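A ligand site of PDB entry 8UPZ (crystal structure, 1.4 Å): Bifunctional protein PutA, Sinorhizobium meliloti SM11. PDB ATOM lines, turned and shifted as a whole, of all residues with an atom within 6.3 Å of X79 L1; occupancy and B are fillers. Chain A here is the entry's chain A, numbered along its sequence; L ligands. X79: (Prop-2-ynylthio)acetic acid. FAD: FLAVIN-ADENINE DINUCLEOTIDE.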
ATOM      1  N   ASP A  95      -6.319  24.903  -7.528  1.00  0.00           N
ATOM      2  CA  ASP A  95      -5.518  25.800  -6.712  1.00  0.00           C
ATOM      3  C   ASP A  95      -5.777  27.217  -7.181  1.00  0.00           C
ATOM      4  O   ASP A  95      -5.276  27.622  -8.241  1.00  0.00           O
ATOM      5  CB  ASP A  95      -4.037  25.442  -6.901  1.00  0.00           C
ATOM      6  CG  ASP A  95      -3.118  26.506  -6.376  1.00  0.00           C
ATOM      7  OD1 ASP A  95      -3.459  27.100  -5.331  1.00  0.00           O
ATOM      8  OD2 ASP A  95      -2.060  26.751  -7.015  1.00  0.00           O
ATOM      9  N   GLU A  99      -0.476  33.573  -2.597  1.00  0.00           N
ATOM     10  CA  GLU A  99       0.307  33.056  -1.474  1.00  0.00           C
ATOM     11  C   GLU A  99       1.013  34.221  -0.806  1.00  0.00           C
ATOM     12  O   GLU A  99       1.108  35.319  -1.360  1.00  0.00           O
ATOM     13  CB  GLU A  99       1.309  32.000  -1.932  1.00  0.00           C
ATOM     14  CG  GLU A  99       2.398  32.502  -2.865  1.00  0.00           C
ATOM     15  CD  GLU A  99       3.253  31.356  -3.356  1.00  0.00           C
ATOM     16  OE1 GLU A  99       2.717  30.437  -4.011  1.00  0.00           O
ATOM     17  OE2 GLU A  99       4.460  31.363  -3.052  1.00  0.00           O
ATOM     18  N   LYS A 139      -3.269  27.343   0.452  1.00  0.00           N
ATOM     19  CA  LYS A 139      -2.009  27.653   1.119  1.00  0.00           C
ATOM     20  C   LYS A 139      -2.304  28.527   2.334  1.00  0.00           C
ATOM     21  O   LYS A 139      -2.951  29.568   2.209  1.00  0.00           O
ATOM     22  CB  LYS A 139      -1.034  28.370   0.176  1.00  0.00           C
ATOM     23  CG  LYS A 139      -0.285  27.424  -0.751  1.00  0.00           C
ATOM     24  CD  LYS A 139       0.607  28.202  -1.721  1.00  0.00           C
ATOM     25  CE  LYS A 139       1.515  27.272  -2.532  1.00  0.00           C
ATOM     26  NZ  LYS A 139       0.751  26.417  -3.490  1.00  0.00           N
ATOM     27  N   ASP A 180      -1.674  22.701   1.284  1.00  0.00           N
ATOM     28  CA  ASP A 180      -0.347  22.586   0.667  1.00  0.00           C
ATOM     29  C   ASP A 180       0.747  22.802   1.718  1.00  0.00           C
ATOM     30  O   ASP A 180       0.564  23.556   2.679  1.00  0.00           O
ATOM     31  CB  ASP A 180      -0.165  23.659  -0.413  1.00  0.00           C
ATOM     32  CG  ASP A 180      -0.949  23.363  -1.696  1.00  0.00           C
ATOM     33  OD1 ASP A 180      -1.527  22.267  -1.857  1.00  0.00           O
ATOM     34  OD2 ASP A 180      -0.968  24.266  -2.557  1.00  0.00           O
ATOM     35  N   ALA A 181       1.882  22.143   1.530  1.00  0.00           N
ATOM     36  CA  ALA A 181       3.043  22.366   2.403  1.00  0.00           C
ATOM     37  C   ALA A 181       3.937  23.460   1.823  1.00  0.00           C
ATOM     38  O   ALA A 181       4.243  23.449   0.628  1.00  0.00           O
ATOM     39  CB  ALA A 181       3.849  21.090   2.532  1.00  0.00           C
ATOM     40  N   GLU A 182       4.373  24.373   2.690  1.00  0.00           N
ATOM     41  CA  GLU A 182       5.216  25.467   2.227  1.00  0.00           C
ATOM     42  C   GLU A 182       6.605  25.392   2.858  1.00  0.00           C
ATOM     43  O   GLU A 182       7.252  24.347   2.761  1.00  0.00           O
ATOM     44  CB  GLU A 182       4.493  26.814   2.417  1.00  0.00           C
ATOM     45  CG  GLU A 182       3.175  26.871   1.636  1.00  0.00           C
ATOM     46  CD  GLU A 182       2.430  28.178   1.856  1.00  0.00           C
ATOM     47  OE1 GLU A 182       2.811  29.194   1.234  1.00  0.00           O
ATOM     48  OE2 GLU A 182       1.452  28.189   2.648  1.00  0.00           O
ATOM     49  N   ARG A 241      -0.933  13.779   0.891  1.00  0.00           N
ATOM     50  CA  ARG A 241      -0.193  13.953  -0.355  1.00  0.00           C
ATOM     51  C   ARG A 241       1.297  13.889  -0.047  1.00  0.00           C
ATOM     52  O   ARG A 241       1.824  14.750   0.655  1.00  0.00           O
ATOM     53  CB  ARG A 241      -0.549  15.276  -1.033  1.00  0.00           C
ATOM     54  CG  ARG A 241       0.210  15.449  -2.352  1.00  0.00           C
ATOM     55  CD  ARG A 241       0.216  16.863  -2.870  1.00  0.00           C
ATOM     56  NE  ARG A 241      -1.135  17.323  -3.201  1.00  0.00           N
ATOM     57  CZ  ARG A 241      -1.520  18.586  -3.185  1.00  0.00           C
ATOM     58  NH1 ARG A 241      -0.678  19.580  -2.880  1.00  0.00           N
ATOM     59  NH2 ARG A 241      -2.782  18.874  -3.499  1.00  0.00           N
ATOM     60  N   ALA A 246       8.902  21.543  -3.091  1.00  0.00           N
ATOM     61  CA  ALA A 246       9.015  22.581  -4.117  1.00  0.00           C
ATOM     62  C   ALA A 246       9.943  23.732  -3.757  1.00  0.00           C
ATOM     63  O   ALA A 246      10.179  24.594  -4.608  1.00  0.00           O
ATOM     64  CB  ALA A 246       7.634  23.173  -4.433  1.00  0.00           C
ATOM     65  N   TYR A 247      10.471  23.785  -2.527  1.00  0.00           N
ATOM     66  CA  TYR A 247      11.168  24.969  -2.019  1.00  0.00           C
ATOM     67  C   TYR A 247      12.637  24.683  -1.707  1.00  0.00           C
ATOM     68  O   TYR A 247      13.240  25.384  -0.885  1.00  0.00           O
ATOM     69  CB  TYR A 247      10.467  25.527  -0.787  1.00  0.00           C
ATOM     70  CG  TYR A 247       8.995  25.829  -0.986  1.00  0.00           C
ATOM     71  CD1 TYR A 247       8.048  24.830  -0.948  1.00  0.00           C
ATOM     72  CD2 TYR A 247       8.549  27.136  -1.182  1.00  0.00           C
ATOM     73  CE1 TYR A 247       6.701  25.098  -1.133  1.00  0.00           C
ATOM     74  CE2 TYR A 247       7.194  27.420  -1.355  1.00  0.00           C
ATOM     75  CZ  TYR A 247       6.284  26.397  -1.333  1.00  0.00           C
ATOM     76  OH  TYR A 247       4.946  26.669  -1.509  1.00  0.00           O
ATOM     77  N   LEU A 323       1.143  17.648 -11.584  1.00  0.00           N
ATOM     78  CA  LEU A 323       0.845  19.052 -11.868  1.00  0.00           C
ATOM     79  C   LEU A 323       0.323  19.227 -13.291  1.00  0.00           C
ATOM     80  O   LEU A 323       0.844  18.630 -14.245  1.00  0.00           O
ATOM     81  CB  LEU A 323       2.084  19.929 -11.676  1.00  0.00           C
ATOM     82  CG  LEU A 323       2.720  19.914 -10.272  1.00  0.00           C
ATOM     83  CD1 LEU A 323       3.944  20.845 -10.185  1.00  0.00           C
ATOM     84  CD2 LEU A 323       1.711  20.301  -9.233  1.00  0.00           C
ATOM     85  N   TYR A 347      -3.229  18.625 -10.173  1.00  0.00           N
ATOM     86  CA  TYR A 347      -3.201  19.869  -9.436  1.00  0.00           C
ATOM     87  C   TYR A 347      -3.319  20.985 -10.471  1.00  0.00           C
ATOM     88  O   TYR A 347      -2.472  21.111 -11.359  1.00  0.00           O
ATOM     89  CB  TYR A 347      -1.884  19.952  -8.663  1.00  0.00           C
ATOM     90  CG  TYR A 347      -1.757  21.128  -7.710  1.00  0.00           C
ATOM     91  CD1 TYR A 347      -1.319  22.362  -8.169  1.00  0.00           C
ATOM     92  CD2 TYR A 347      -2.050  20.995  -6.347  1.00  0.00           C
ATOM     93  CE1 TYR A 347      -1.210  23.439  -7.323  1.00  0.00           C
ATOM     94  CE2 TYR A 347      -1.936  22.084  -5.481  1.00  0.00           C
ATOM     95  CZ  TYR A 347      -1.510  23.293  -5.981  1.00  0.00           C
ATOM     96  OH  TYR A 347      -1.362  24.382  -5.139  1.00  0.00           O
ATOM     97  N   ALA A 358       4.864  33.487  -8.650  1.00  0.00           N
ATOM     98  CA  ALA A 358       5.618  32.749  -7.643  1.00  0.00           C
ATOM     99  C   ALA A 358       5.598  31.258  -7.927  1.00  0.00           C
ATOM    100  O   ALA A 358       6.612  30.563  -7.781  1.00  0.00           O
ATOM    101  CB  ALA A 358       5.036  33.016  -6.256  1.00  0.00           C
ATOM    102  N   TYR A 359       4.426  30.746  -8.288  1.00  0.00           N
ATOM    103  CA  TYR A 359       4.299  29.349  -8.683  1.00  0.00           C
ATOM    104  C   TYR A 359       5.200  29.051  -9.875  1.00  0.00           C
ATOM    105  O   TYR A 359       5.898  28.024  -9.895  1.00  0.00           O
ATOM    106  CB  TYR A 359       2.822  29.071  -8.982  1.00  0.00           C
ATOM    107  CG  TYR A 359       2.464  27.671  -9.383  1.00  0.00           C
ATOM    108  CD1 TYR A 359       2.435  27.304 -10.723  1.00  0.00           C
ATOM    109  CD2 TYR A 359       2.099  26.721  -8.434  1.00  0.00           C
ATOM    110  CE1 TYR A 359       2.095  26.016 -11.107  1.00  0.00           C
ATOM    111  CE2 TYR A 359       1.768  25.437  -8.809  1.00  0.00           C
ATOM    112  CZ  TYR A 359       1.756  25.102 -10.138  1.00  0.00           C
ATOM    113  OH  TYR A 359       1.406  23.814 -10.480  1.00  0.00           O
ATOM    114  N   ARG A 362       8.882  28.422  -8.972  1.00  0.00           N
ATOM    115  CA  ARG A 362       9.145  27.082  -8.457  1.00  0.00           C
ATOM    116  C   ARG A 362       9.102  26.046  -9.568  1.00  0.00           C
ATOM    117  O   ARG A 362       9.889  25.089  -9.552  1.00  0.00           O
ATOM    118  CB  ARG A 362       8.195  26.743  -7.303  1.00  0.00           C
ATOM    119  CG  ARG A 362       8.438  27.608  -6.066  1.00  0.00           C
ATOM    120  CD  ARG A 362       7.629  27.169  -4.875  1.00  0.00           C
ATOM    121  NE  ARG A 362       6.202  27.351  -5.100  1.00  0.00           N
ATOM    122  CZ  ARG A 362       5.538  28.463  -4.824  1.00  0.00           C
ATOM    123  NH1 ARG A 362       6.124  29.506  -4.265  1.00  0.00           N
ATOM    124  NH2 ARG A 362       4.237  28.525  -5.092  1.00  0.00           N
ATOM    125  N   ARG A 363       8.242  26.248 -10.579  1.00  0.00           N
ATOM    126  CA  ARG A 363       8.241  25.334 -11.725  1.00  0.00           C
ATOM    127  C   ARG A 363       9.514  25.450 -12.549  1.00  0.00           C
ATOM    128  O   ARG A 363       9.998  24.459 -13.098  1.00  0.00           O
ATOM    129  CB  ARG A 363       7.013  25.585 -12.612  1.00  0.00           C
ATOM    130  CG  ARG A 363       5.661  25.415 -11.885  1.00  0.00           C
ATOM    131  CD  ARG A 363       5.330  23.971 -11.475  1.00  0.00           C
ATOM    132  NE  ARG A 363       6.023  23.519 -10.276  1.00  0.00           N
ATOM    133  CZ  ARG A 363       5.799  23.969  -9.053  1.00  0.00           C
ATOM    134  NH1 ARG A 363       4.923  24.944  -8.827  1.00  0.00           N
ATOM    135  NH2 ARG A 363       6.443  23.422  -8.038  1.00  0.00           N
ATOM    136  N   GLU A 366      12.159  23.588 -10.750  1.00  0.00           N
ATOM    137  CA  GLU A 366      11.896  22.154 -10.861  1.00  0.00           C
ATOM    138  C   GLU A 366      12.243  21.651 -12.263  1.00  0.00           C
ATOM    139  O   GLU A 366      12.924  20.622 -12.413  1.00  0.00           O
ATOM    140  CB  GLU A 366      10.427  21.884 -10.544  1.00  0.00           C
ATOM    141  CG  GLU A 366       9.956  20.460 -10.744  1.00  0.00           C
ATOM    142  CD  GLU A 366       8.496  20.302 -10.368  1.00  0.00           C
ATOM    143  OE1 GLU A 366       7.826  21.328 -10.078  1.00  0.00           O
ATOM    144  OE2 GLU A 366       8.008  19.150 -10.351  1.00  0.00           O
HETATM  145  C01 X79 L   1       3.140  22.229  -6.500  1.00  0.00           C
HETATM  146  C02 X79 L   1       2.422  22.501  -5.603  1.00  0.00           C
HETATM  147  C03 X79 L   1       1.566  22.868  -4.541  1.00  0.00           C
HETATM  148  C05 X79 L   1       4.206  24.383  -3.952  1.00  0.00           C
HETATM  149  C06 X79 L   1       3.974  25.229  -5.249  1.00  0.00           C
HETATM  150  O07 X79 L   1       2.895  25.844  -5.334  1.00  0.00           O
HETATM  151  O08 X79 L   1       4.878  25.198  -6.116  1.00  0.00           O
HETATM  152  S04 X79 L   1       2.586  23.737  -3.236  1.00  0.00           S
HETATM  153  PA  FAD L   2      12.195  14.299  -9.230  1.00  0.00           P
HETATM  154  O1A FAD L   2      12.996  14.818 -10.373  1.00  0.00           O
HETATM  155  O2A FAD L   2      12.307  12.815  -8.963  1.00  0.00           O
HETATM  156  O5B FAD L   2      12.529  14.995  -7.916  1.00  0.00           O
HETATM  157  C5B FAD L   2      12.858  16.408  -7.874  1.00  0.00           C
HETATM  158  C4B FAD L   2      12.825  16.890  -6.447  1.00  0.00           C
HETATM  159  O4B FAD L   2      13.983  16.424  -5.723  1.00  0.00           O
HETATM  160  C3B FAD L   2      12.866  18.395  -6.265  1.00  0.00           C
HETATM  161  O3B FAD L   2      11.574  18.938  -6.534  1.00  0.00           O
HETATM  162  C2B FAD L   2      13.285  18.501  -4.787  1.00  0.00           C
HETATM  163  O2B FAD L   2      12.214  18.224  -3.898  1.00  0.00           O
HETATM  164  C1B FAD L   2      14.290  17.340  -4.670  1.00  0.00           C
HETATM  165  N9A FAD L   2      15.700  17.711  -4.790  1.00  0.00           N
HETATM  166  C8A FAD L   2      16.330  18.229  -5.885  1.00  0.00           C
HETATM  167  N7A FAD L   2      17.617  18.441  -5.713  1.00  0.00           N
HETATM  168  C5A FAD L   2      17.854  18.006  -4.423  1.00  0.00           C
HETATM  169  C6A FAD L   2      19.015  17.939  -3.635  1.00  0.00           C
HETATM  170  N6A FAD L   2      20.222  18.330  -4.055  1.00  0.00           N
HETATM  171  N1A FAD L   2      18.895  17.456  -2.381  1.00  0.00           N
HETATM  172  C2A FAD L   2      17.699  17.047  -1.953  1.00  0.00           C
HETATM  173  N3A FAD L   2      16.528  17.065  -2.602  1.00  0.00           N
HETATM  174  C4A FAD L   2      16.677  17.539  -3.840  1.00  0.00           C
HETATM  175  N1  FAD L   2       5.831  20.439  -3.014  1.00  0.00           N
HETATM  176  C2  FAD L   2       5.697  21.147  -1.861  1.00  0.00           C
HETATM  177  O2  FAD L   2       6.689  21.592  -1.264  1.00  0.00           O
HETATM  178  N3  FAD L   2       4.414  21.412  -1.377  1.00  0.00           N
HETATM  179  C4  FAD L   2       3.228  21.003  -1.950  1.00  0.00           C
HETATM  180  O4  FAD L   2       2.150  21.261  -1.408  1.00  0.00           O
HETATM  181  C4X FAD L   2       3.395  20.232  -3.173  1.00  0.00           C
HETATM  182  N5  FAD L   2       2.297  19.787  -3.788  1.00  0.00           N
HETATM  183  C5X FAD L   2       2.473  19.046  -4.949  1.00  0.00           C
HETATM  184  C6  FAD L   2       1.353  18.574  -5.625  1.00  0.00           C
HETATM  185  C7  FAD L   2       1.485  17.808  -6.783  1.00  0.00           C
HETATM  186  C7M FAD L   2       0.248  17.295  -7.480  1.00  0.00           C
HETATM  187  C8  FAD L   2       2.768  17.521  -7.279  1.00  0.00           C
HETATM  188  C8M FAD L   2       2.956  16.709  -8.538  1.00  0.00           C
HETATM  189  C9  FAD L   2       3.890  18.009  -6.622  1.00  0.00           C
HETATM  190  C9A FAD L   2       3.754  18.761  -5.464  1.00  0.00           C
HETATM  191  N10 FAD L   2       4.879  19.284  -4.795  1.00  0.00           N
HETATM  192  C10 FAD L   2       4.730  19.980  -3.620  1.00  0.00           C
HETATM  193  C1' FAD L   2       6.234  18.863  -5.198  1.00  0.00           C
HETATM  194  C2' FAD L   2       6.985  19.809  -6.118  1.00  0.00           C
HETATM  195  O2' FAD L   2       6.126  20.772  -6.702  1.00  0.00           O
HETATM  196  C3' FAD L   2       7.645  18.977  -7.228  1.00  0.00           C
HETATM  197  O3' FAD L   2       6.649  18.678  -8.205  1.00  0.00           O
HETATM  198  C4' FAD L   2       8.303  17.666  -6.803  1.00  0.00           C
HETATM  199  O4' FAD L   2       9.120  17.850  -5.655  1.00  0.00           O
HETATM  200  C5' FAD L   2       9.057  17.008  -7.939  1.00  0.00           C
HETATM  201  O5' FAD L   2       9.281  15.616  -7.625  1.00  0.00           O
HETATM  202  P   FAD L   2       9.254  14.510  -8.744  1.00  0.00           P
HETATM  203  O1P FAD L   2       9.214  13.154  -8.036  1.00  0.00           O
HETATM  204  O2P FAD L   2       8.249  14.807  -9.711  1.00  0.00           O
HETATM  205  O3P FAD L   2      10.679  14.674  -9.459  1.00  0.00           O
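NH1 of Arg 363 is in salt-bridge range of O08 of X79 L1 (2.7 Å).
An oxygen (O08) of X79 L1 is in salt-bridge range of the guanidinium group (NE) of Arg 362, 2.7 Å away.
O07 of X79 L1 lies within salt-bridge range of NZ of Lys 139, at 2.9 Å.
NH2 of Arg 363 is in hydrogen-bond range of O2' of FAD L2, 3.0 Å away.
O2 of FAD L2 is in hydrogen-bond range of N of Ala 246 (2.9 Å).
The backbone NH (N) of Ala 181 lies within hydrogen-bond range of an oxygen (O4) of FAD L2 (3.1 Å).
The backbone carbonyl oxygen of Ala 181 lies within hydrogen-bond range of a nitrogen (N3) of FAD L2, 2.9 Å away.
N5 of FAD L2 lies within hydrogen-bond range of NH1 of Arg 241 (3.1 Å).
O3' of FAD L2 sits at hydrogen-bond distance from OE2 of Glu 366 (2.6 Å).
A sulfur (S04) of X79 L1 sits close to a nitrogen (N3) of FAD L2 (3.5 Å).
The guanidinium group (NH1) of Arg 363 sits close to the backbone carbonyl oxygen (O) of Tyr 359, 3.4 Å away.
NE of Arg 363 is in salt-bridge range of OE1 of Glu 366 (2.8 Å).
NH2 of Arg 362 lies within salt-bridge range of OE1 of Glu 99, at 2.7 Å.
The side-chain amino group (NZ) of Lys 139 lies within hydrogen-bond range of the side-chain hydroxyl (OH) of Tyr 347, 3.4 Å away.
OD2 of Asp 180 is in salt-bridge range of NZ of Lys 139 (2.9 Å).
OH of Tyr 347 sits at hydrogen-bond distance from OD2 of Asp 180.
The side-chain hydroxyl (OH) of Tyr 347 lies close to the side-chain carboxylate (OD2) of Asp 95.
OD1 of Asp 180 is in salt-bridge range of NH1 of Arg 241 (3.0 Å).
OD2 of Asp 180 sits close to S04 of X79 L1.
CB of Ala 246 touches C05 of X79 L1, at 3.7 Å.
Tyr 247 touches X79 L1 (OH to C05, 3.4 Å).
Leu 323 touches X79 L1.
Tyr 347 touches X79 L1.
CD2 of Tyr 359 touches O07 of X79 L1 (3.3 Å).
Hydrophobic or aromatic side chains that line X79 L1: Ala 246, Tyr 247, Leu 323, Tyr 347 and Tyr 359.
Of the 16 residues printed, 9 come within 4 Å of X79 L1.
The nearest printed residue that does not touch X79 L1 is Ala 181 (4.2 Å).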
